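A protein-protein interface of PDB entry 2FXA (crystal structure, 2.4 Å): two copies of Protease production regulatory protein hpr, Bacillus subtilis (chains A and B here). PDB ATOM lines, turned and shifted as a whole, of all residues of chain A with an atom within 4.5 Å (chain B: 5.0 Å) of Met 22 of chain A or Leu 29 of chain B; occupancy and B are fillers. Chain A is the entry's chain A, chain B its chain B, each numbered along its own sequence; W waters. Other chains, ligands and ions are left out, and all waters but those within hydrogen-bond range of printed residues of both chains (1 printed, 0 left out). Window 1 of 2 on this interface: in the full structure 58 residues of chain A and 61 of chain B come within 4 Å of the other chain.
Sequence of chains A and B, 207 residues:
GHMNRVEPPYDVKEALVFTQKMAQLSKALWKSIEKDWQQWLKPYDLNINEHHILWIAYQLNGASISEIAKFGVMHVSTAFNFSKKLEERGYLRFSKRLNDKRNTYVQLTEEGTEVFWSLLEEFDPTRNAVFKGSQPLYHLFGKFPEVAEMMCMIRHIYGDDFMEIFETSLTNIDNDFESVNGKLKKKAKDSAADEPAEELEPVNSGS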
ATOM      1  N   PHE A  18      39.327   1.367  27.664  1.00  0.00           N
ATOM      2  CA  PHE A  18      38.100   0.796  27.133  1.00  0.00           C
ATOM      3  C   PHE A  18      37.039   1.854  26.801  1.00  0.00           C
ATOM      4  O   PHE A  18      36.458   1.873  25.729  1.00  0.00           O
ATOM      5  CB  PHE A  18      37.544  -0.236  28.110  1.00  0.00           C
ATOM      6  CG  PHE A  18      36.213  -0.769  27.700  1.00  0.00           C
ATOM      7  CD1 PHE A  18      36.096  -1.608  26.573  1.00  0.00           C
ATOM      8  CD2 PHE A  18      35.076  -0.416  28.395  1.00  0.00           C
ATOM      9  CE1 PHE A  18      34.857  -2.105  26.183  1.00  0.00           C
ATOM     10  CE2 PHE A  18      33.818  -0.910  28.012  1.00  0.00           C
ATOM     11  CZ  PHE A  18      33.708  -1.748  26.924  1.00  0.00           C
ATOM     12  N   THR A  19      36.790   2.723  27.762  1.00  0.00           N
ATOM     13  CA  THR A  19      35.883   3.842  27.649  1.00  0.00           C
ATOM     14  C   THR A  19      36.189   4.743  26.452  1.00  0.00           C
ATOM     15  O   THR A  19      35.314   5.110  25.711  1.00  0.00           O
ATOM     16  CB  THR A  19      35.972   4.622  29.011  1.00  0.00           C
ATOM     17  OG1 THR A  19      35.293   3.854  30.005  1.00  0.00           O
ATOM     18  CG2 THR A  19      35.345   5.971  28.969  1.00  0.00           C
ATOM     19  N   GLN A  20      37.442   5.098  26.243  1.00  0.00           N
ATOM     20  CA  GLN A  20      37.776   5.914  25.103  1.00  0.00           C
ATOM     21  C   GLN A  20      37.749   5.124  23.771  1.00  0.00           C
ATOM     22  O   GLN A  20      37.433   5.696  22.719  1.00  0.00           O
ATOM     23  CB  GLN A  20      39.069   6.722  25.385  1.00  0.00           C
ATOM     24  CG  GLN A  20      40.358   5.952  25.260  1.00  0.00           C
ATOM     25  CD  GLN A  20      41.579   6.653  25.984  1.00  0.00           C
ATOM     26  OE1 GLN A  20      42.746   6.370  25.691  1.00  0.00           O
ATOM     27  NE2 GLN A  20      41.281   7.551  26.916  1.00  0.00           N
ATOM     28  N   LYS A  21      38.028   3.818  23.805  1.00  0.00           N
ATOM     29  CA  LYS A  21      37.863   2.989  22.614  1.00  0.00           C
ATOM     30  C   LYS A  21      36.366   2.958  22.240  1.00  0.00           C
ATOM     31  O   LYS A  21      36.003   3.240  21.124  1.00  0.00           O
ATOM     32  CB  LYS A  21      38.469   1.582  22.816  1.00  0.00           C
ATOM     33  CG  LYS A  21      37.837   0.437  21.966  1.00  0.00           C
ATOM     34  CD  LYS A  21      38.530  -0.939  22.144  1.00  0.00           C
ATOM     35  CE  LYS A  21      37.623  -2.149  21.741  1.00  0.00           C
ATOM     36  NZ  LYS A  21      38.438  -3.405  21.484  1.00  0.00           N
ATOM     37  N   MET A  22      35.503   2.713  23.200  1.00  0.00           N
ATOM     38  CA  MET A  22      34.048   2.748  22.955  1.00  0.00           C
ATOM     39  C   MET A  22      33.557   4.081  22.412  1.00  0.00           C
ATOM     40  O   MET A  22      32.839   4.091  21.409  1.00  0.00           O
ATOM     41  CB  MET A  22      33.250   2.320  24.193  1.00  0.00           C
ATOM     42  CG  MET A  22      33.545   0.932  24.588  1.00  0.00           C
ATOM     43  SD  MET A  22      33.277  -0.429  23.104  1.00  0.00           S
ATOM     44  CE  MET A  22      31.473   0.161  22.445  1.00  0.00           C
ATOM     45  N   ALA A  23      34.004   5.193  23.003  1.00  0.00           N
ATOM     46  CA  ALA A  23      33.645   6.530  22.485  1.00  0.00           C
ATOM     47  C   ALA A  23      34.059   6.733  21.044  1.00  0.00           C
ATOM     48  O   ALA A  23      33.294   7.185  20.194  1.00  0.00           O
ATOM     49  CB  ALA A  23      34.228   7.642  23.374  1.00  0.00           C
ATOM     50  N   GLN A  24      35.285   6.413  20.749  1.00  0.00           N
ATOM     51  CA  GLN A  24      35.786   6.569  19.417  1.00  0.00           C
ATOM     52  C   GLN A  24      35.040   5.709  18.347  1.00  0.00           C
ATOM     53  O   GLN A  24      34.681   6.208  17.265  1.00  0.00           O
ATOM     54  CB  GLN A  24      37.269   6.172  19.487  1.00  0.00           C
ATOM     55  CG  GLN A  24      38.016   6.289  18.209  1.00  0.00           C
ATOM     56  CD  GLN A  24      38.462   7.701  17.931  1.00  0.00           C
ATOM     57  OE1 GLN A  24      38.293   8.624  18.752  1.00  0.00           O
ATOM     58  NE2 GLN A  24      39.043   7.884  16.764  1.00  0.00           N
ATOM     59  N   LEU A  25      34.842   4.422  18.636  1.00  0.00           N
ATOM     60  CA  LEU A  25      34.159   3.512  17.708  1.00  0.00           C
ATOM     61  C   LEU A  25      32.707   3.934  17.530  1.00  0.00           C
ATOM     62  O   LEU A  25      32.161   3.957  16.452  1.00  0.00           O
ATOM     63  CB  LEU A  25      34.179   2.091  18.279  1.00  0.00           C
ATOM     64  CG  LEU A  25      35.524   1.342  18.269  1.00  0.00           C
ATOM     65  CD1 LEU A  25      35.325   0.003  18.959  1.00  0.00           C
ATOM     66  CD2 LEU A  25      36.101   1.156  16.846  1.00  0.00           C
ATOM     67  N   SER A  26      32.114   4.320  18.628  1.00  0.00           N
ATOM     68  CA  SER A  26      30.763   4.650  18.662  1.00  0.00           C
ATOM     69  C   SER A  26      30.464   5.972  17.906  1.00  0.00           C
ATOM     70  O   SER A  26      29.462   6.075  17.156  1.00  0.00           O
ATOM     71  CB  SER A  26      30.372   4.626  20.143  1.00  0.00           C
ATOM     72  OG  SER A  26      29.234   5.362  20.376  1.00  0.00           O
ATOM     73  N   MET A 150      27.790  -5.532  21.680  1.00  0.00           N
ATOM     74  CA  MET A 150      27.149  -4.240  21.560  1.00  0.00           C
ATOM     75  C   MET A 150      25.691  -4.253  22.052  1.00  0.00           C
ATOM     76  O   MET A 150      25.285  -3.393  22.804  1.00  0.00           O
ATOM     77  CB  MET A 150      27.218  -3.824  20.117  1.00  0.00           C
ATOM     78  CG  MET A 150      27.180  -2.352  19.917  1.00  0.00           C
ATOM     79  SD  MET A 150      26.842  -1.902  18.005  1.00  0.00           S
ATOM     80  CE  MET A 150      26.349   0.111  18.256  1.00  0.00           C
ATOM     81  N   MET A 153      25.451  -4.552  25.916  1.00  0.00           N
ATOM     82  CA  MET A 153      25.729  -3.273  26.569  1.00  0.00           C
ATOM     83  C   MET A 153      24.506  -2.333  26.504  1.00  0.00           C
ATOM     84  O   MET A 153      24.100  -1.749  27.506  1.00  0.00           O
ATOM     85  CB  MET A 153      26.960  -2.600  25.971  1.00  0.00           C
ATOM     86  CG  MET A 153      28.254  -3.362  26.144  1.00  0.00           C
ATOM     87  SD  MET A 153      29.788  -2.480  25.146  1.00  0.00           S
ATOM     88  CE  MET A 153      28.837  -1.714  23.769  1.00  0.00           C
ATOM     89  N   ILE A 154      23.925  -2.227  25.319  1.00  0.00           N
ATOM     90  CA  ILE A 154      22.746  -1.424  25.098  1.00  0.00           C
ATOM     91  C   ILE A 154      21.589  -1.912  25.973  1.00  0.00           C
ATOM     92  O   ILE A 154      20.898  -1.084  26.561  1.00  0.00           O
ATOM     93  CB  ILE A 154      22.375  -1.376  23.597  1.00  0.00           C
ATOM     94  CG1 ILE A 154      23.405  -0.570  22.804  1.00  0.00           C
ATOM     95  CG2 ILE A 154      20.971  -0.807  23.344  1.00  0.00           C
ATOM     96  CD1 ILE A 154      23.839   0.722  23.476  1.00  0.00           C
ATOM     97  N   LEU B  25      21.068   0.728  17.323  1.00  0.00           N
ATOM     98  CA  LEU B  25      22.082   0.390  18.331  1.00  0.00           C
ATOM     99  C   LEU B  25      23.129   1.504  18.394  1.00  0.00           C
ATOM    100  O   LEU B  25      23.565   1.983  19.419  1.00  0.00           O
ATOM    101  CB  LEU B  25      22.786  -0.888  17.886  1.00  0.00           C
ATOM    102  CG  LEU B  25      22.487  -2.261  18.483  1.00  0.00           C
ATOM    103  CD1 LEU B  25      21.240  -2.320  19.383  1.00  0.00           C
ATOM    104  CD2 LEU B  25      22.510  -3.347  17.428  1.00  0.00           C
ATOM    105  N   SER B  26      23.506   1.949  17.228  1.00  0.00           N
ATOM    106  CA  SER B  26      24.503   2.955  17.115  1.00  0.00           C
ATOM    107  C   SER B  26      24.060   4.328  17.672  1.00  0.00           C
ATOM    108  O   SER B  26      24.865   5.013  18.309  1.00  0.00           O
ATOM    109  CB  SER B  26      24.878   2.993  15.649  1.00  0.00           C
ATOM    110  OG  SER B  26      25.460   4.191  15.322  1.00  0.00           O
ATOM    111  N   LYS B  27      22.807   4.732  17.441  1.00  0.00           N
ATOM    112  CA  LYS B  27      22.289   5.970  18.032  1.00  0.00           C
ATOM    113  C   LYS B  27      22.213   5.842  19.551  1.00  0.00           C
ATOM    114  O   LYS B  27      22.607   6.746  20.273  1.00  0.00           O
ATOM    115  CB  LYS B  27      20.901   6.347  17.442  1.00  0.00           C
ATOM    116  CG  LYS B  27      20.383   7.761  17.805  1.00  0.00           C
ATOM    117  CD  LYS B  27      18.979   8.002  17.219  1.00  0.00           C
ATOM    118  CE  LYS B  27      18.503   9.427  17.500  1.00  0.00           C
ATOM    119  NZ  LYS B  27      17.050   9.605  17.095  1.00  0.00           N
ATOM    120  N   ALA B  28      21.742   4.697  20.031  1.00  0.00           N
ATOM    121  CA  ALA B  28      21.624   4.437  21.441  1.00  0.00           C
ATOM    122  C   ALA B  28      22.979   4.510  22.168  1.00  0.00           C
ATOM    123  O   ALA B  28      23.080   5.108  23.226  1.00  0.00           O
ATOM    124  CB  ALA B  28      20.951   3.044  21.667  1.00  0.00           C
ATOM    125  N   LEU B  29      23.987   3.837  21.627  1.00  0.00           N
ATOM    126  CA  LEU B  29      25.336   3.830  22.192  1.00  0.00           C
ATOM    127  C   LEU B  29      25.983   5.236  22.185  1.00  0.00           C
ATOM    128  O   LEU B  29      26.399   5.741  23.197  1.00  0.00           O
ATOM    129  CB  LEU B  29      26.200   2.834  21.384  1.00  0.00           C
ATOM    130  CG  LEU B  29      27.577   2.479  21.953  1.00  0.00           C
ATOM    131  CD1 LEU B  29      27.534   1.947  23.452  1.00  0.00           C
ATOM    132  CD2 LEU B  29      28.235   1.469  21.046  1.00  0.00           C
ATOM    133  N   TRP B  30      26.038   5.885  21.047  1.00  0.00           N
ATOM    134  CA  TRP B  30      26.640   7.195  20.999  1.00  0.00           C
ATOM    135  C   TRP B  30      25.907   8.231  21.879  1.00  0.00           C
ATOM    136  O   TRP B  30      26.559   8.967  22.601  1.00  0.00           O
ATOM    137  CB  TRP B  30      26.773   7.685  19.556  1.00  0.00           C
ATOM    138  CG  TRP B  30      27.173   9.106  19.518  1.00  0.00           C
ATOM    139  CD1 TRP B  30      26.418  10.151  19.101  1.00  0.00           C
ATOM    140  CD2 TRP B  30      28.416   9.663  19.997  1.00  0.00           C
ATOM    141  NE1 TRP B  30      27.103  11.306  19.257  1.00  0.00           N
ATOM    142  CE2 TRP B  30      28.337  11.050  19.798  1.00  0.00           C
ATOM    143  CE3 TRP B  30      29.568   9.121  20.583  1.00  0.00           C
ATOM    144  CZ2 TRP B  30      29.378  11.931  20.162  1.00  0.00           C
ATOM    145  CZ3 TRP B  30      30.635  10.005  20.946  1.00  0.00           C
ATOM    146  CH2 TRP B  30      30.524  11.383  20.728  1.00  0.00           C
ATOM    147  N   LYS B  31      24.572   8.269  21.869  1.00  0.00           N
ATOM    148  CA  LYS B  31      23.862   9.239  22.729  1.00  0.00           C
ATOM    149  C   LYS B  31      24.143   9.036  24.186  1.00  0.00           C
ATOM    150  O   LYS B  31      24.263   9.983  24.930  1.00  0.00           O
ATOM    151  CB  LYS B  31      22.346   9.235  22.504  1.00  0.00           C
ATOM    152  CG  LYS B  31      21.957   9.677  21.091  1.00  0.00           C
ATOM    153  CD  LYS B  31      22.227  11.153  20.855  1.00  0.00           C
ATOM    154  CE  LYS B  31      22.189  11.472  19.375  1.00  0.00           C
ATOM    155  NZ  LYS B  31      22.329  12.956  19.187  1.00  0.00           N
ATOM    156  N   SER B  32      24.247   7.789  24.600  1.00  0.00           N
ATOM    157  CA  SER B  32      24.602   7.478  25.961  1.00  0.00           C
ATOM    158  C   SER B  32      26.030   7.985  26.331  1.00  0.00           C
ATOM    159  O   SER B  32      26.224   8.590  27.367  1.00  0.00           O
ATOM    160  CB  SER B  32      24.515   5.973  26.099  1.00  0.00           C
ATOM    161  OG  SER B  32      25.180   5.544  27.249  1.00  0.00           O
ATOM    162  N   ILE B  33      27.012   7.751  25.462  1.00  0.00           N
ATOM    163  CA  ILE B  33      28.402   8.158  25.681  1.00  0.00           C
ATOM    164  C   ILE B  33      28.521   9.671  25.713  1.00  0.00           C
ATOM    165  O   ILE B  33      29.120  10.227  26.623  1.00  0.00           O
ATOM    166  CB  ILE B  33      29.312   7.540  24.572  1.00  0.00           C
ATOM    167  CG1 ILE B  33      29.460   6.034  24.849  1.00  0.00           C
ATOM    168  CG2 ILE B  33      30.694   8.281  24.449  1.00  0.00           C
ATOM    169  CD1 ILE B  33      30.176   5.316  23.727  1.00  0.00           C
ATOM    170  N   VAL B 130      28.422   3.206  29.795  1.00  0.00           N
ATOM    171  CA  VAL B 130      29.062   2.202  28.974  1.00  0.00           C
ATOM    172  C   VAL B 130      29.958   1.211  29.761  1.00  0.00           C
ATOM    173  O   VAL B 130      29.853   0.009  29.567  1.00  0.00           O
ATOM    174  CB  VAL B 130      29.775   2.846  27.749  1.00  0.00           C
ATOM    175  CG1 VAL B 130      30.587   1.793  26.999  1.00  0.00           C
ATOM    176  CG2 VAL B 130      28.682   3.393  26.806  1.00  0.00           C
ATOM    177  N   VAL B 147      34.576  -6.134  21.160  1.00  0.00           N
ATOM    178  CA  VAL B 147      33.677  -5.626  20.094  1.00  0.00           C
ATOM    179  C   VAL B 147      34.320  -5.744  18.685  1.00  0.00           C
ATOM    180  O   VAL B 147      34.316  -4.809  17.894  1.00  0.00           O
ATOM    181  CB  VAL B 147      33.050  -4.206  20.361  1.00  0.00           C
ATOM    182  CG1 VAL B 147      32.036  -4.238  21.511  1.00  0.00           C
ATOM    183  CG2 VAL B 147      34.118  -3.122  20.569  1.00  0.00           C
ATOM    184  N   MET B 150      32.229  -4.842  15.402  1.00  0.00           N
ATOM    185  CA  MET B 150      32.156  -3.399  15.312  1.00  0.00           C
ATOM    186  C   MET B 150      33.482  -2.800  14.815  1.00  0.00           C
ATOM    187  O   MET B 150      33.493  -1.928  13.977  1.00  0.00           O
ATOM    188  CB  MET B 150      31.811  -2.824  16.682  1.00  0.00           C
ATOM    189  CG  MET B 150      31.418  -1.370  16.660  1.00  0.00           C
ATOM    190  SD  MET B 150      31.033  -0.642  18.511  1.00  0.00           S
ATOM    191  CE  MET B 150      30.497   1.279  18.040  1.00  0.00           C
HETATM  192  O   HOH W   1      27.472   4.242  17.800  1.00  0.00           O
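The side-chain hydroxyl (OG) of Ser 26 of chain A sits close to the backbone NH (N) of Trp 30 of chain B.
Ile 33 of chain B touches Met 22 of chain A (CD1 to O, 3.7 Å). Met 22 of chain A touches Val 130 of chain B (CB to CG1, 3.9 Å). Met 22 of chain A touches Val 147 of chain B. Ala 23 of chain A touches Ile 33 of chain B (CB to CG2, 3.7 Å). Leu 25 of chain A touches Val 147 of chain B (CD1 to CG2, 3.7 Å). Met 150 of chain B touches Ser 26 of chain A. C of Leu 25 of chain B touches CE of Met 150 of chain A (3.5 Å). CE of Met 150 of chain A touches CD2 of Leu 29 of chain B, 3.6 Å away. CE of Met 153 of chain A touches CD1 of Leu 29 of chain B, at 3.9 Å. CD1 of Ile 154 of chain A touches N of Leu 29 of chain B, at 3.6 Å.
Met 22 of chain A touches just these residues of chain B: Leu 29 (3.8 Å), Ile 33 (3.7 Å), Val 130 (3.9 Å) and Val 147 (3.8 Å). Of the printed residues of chain A, Ser 26 of chain B touches Met 150 (3.5 Å). Of the printed residues of chain A, Trp 30 of chain B touches Ala 23 (3.9 Å) and Ser 26 (3.2 Å). Of the printed residues of chain B, Leu 25 of chain A touches Val 147 and Met 150. Printed residues of chain B within 4 Å of Met 150 of chain A: Leu 25, Ser 26 and Leu 29. Lys 31 of chain B touches none of the printed residues of chain A. Gln 24 of chain A touches none of the printed residues of chain B. The nearest residue of chain B that does not touch Met 22 of chain A is Met 150 of chain B (4.04 Å). The nearest printed residue of chain A that does not touch Leu 29 of chain B is Leu 25 of chain A (6.2 Å).
Of the 12 printed residues of chain A, 8 touch a printed residue of chain B. Hydrophobic or aromatic side chains of chain A that line the printed part of chain B: Met 22, Ala 23, Leu 25, Met 150, Met 153 and Ile 154. Of the 12 printed residues of chain B, 8 touch a printed residue of chain A.
Leu 25 of chain A touches Met 150 of chain B, and with the chains exchanged Met 150 of chain A touches Leu 25 of chain B. Ser 26 of chain A touches Met 150 of chain B, and with the chains exchanged Met 150 of chain A touches Ser 26 of chain B. Positions printed for both chains: 25, 26 and 150.
Water W1 bridges O of Ser 26 of chain B (2.8 Å) and O of Ser 26 of chain A (2.8 Å).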
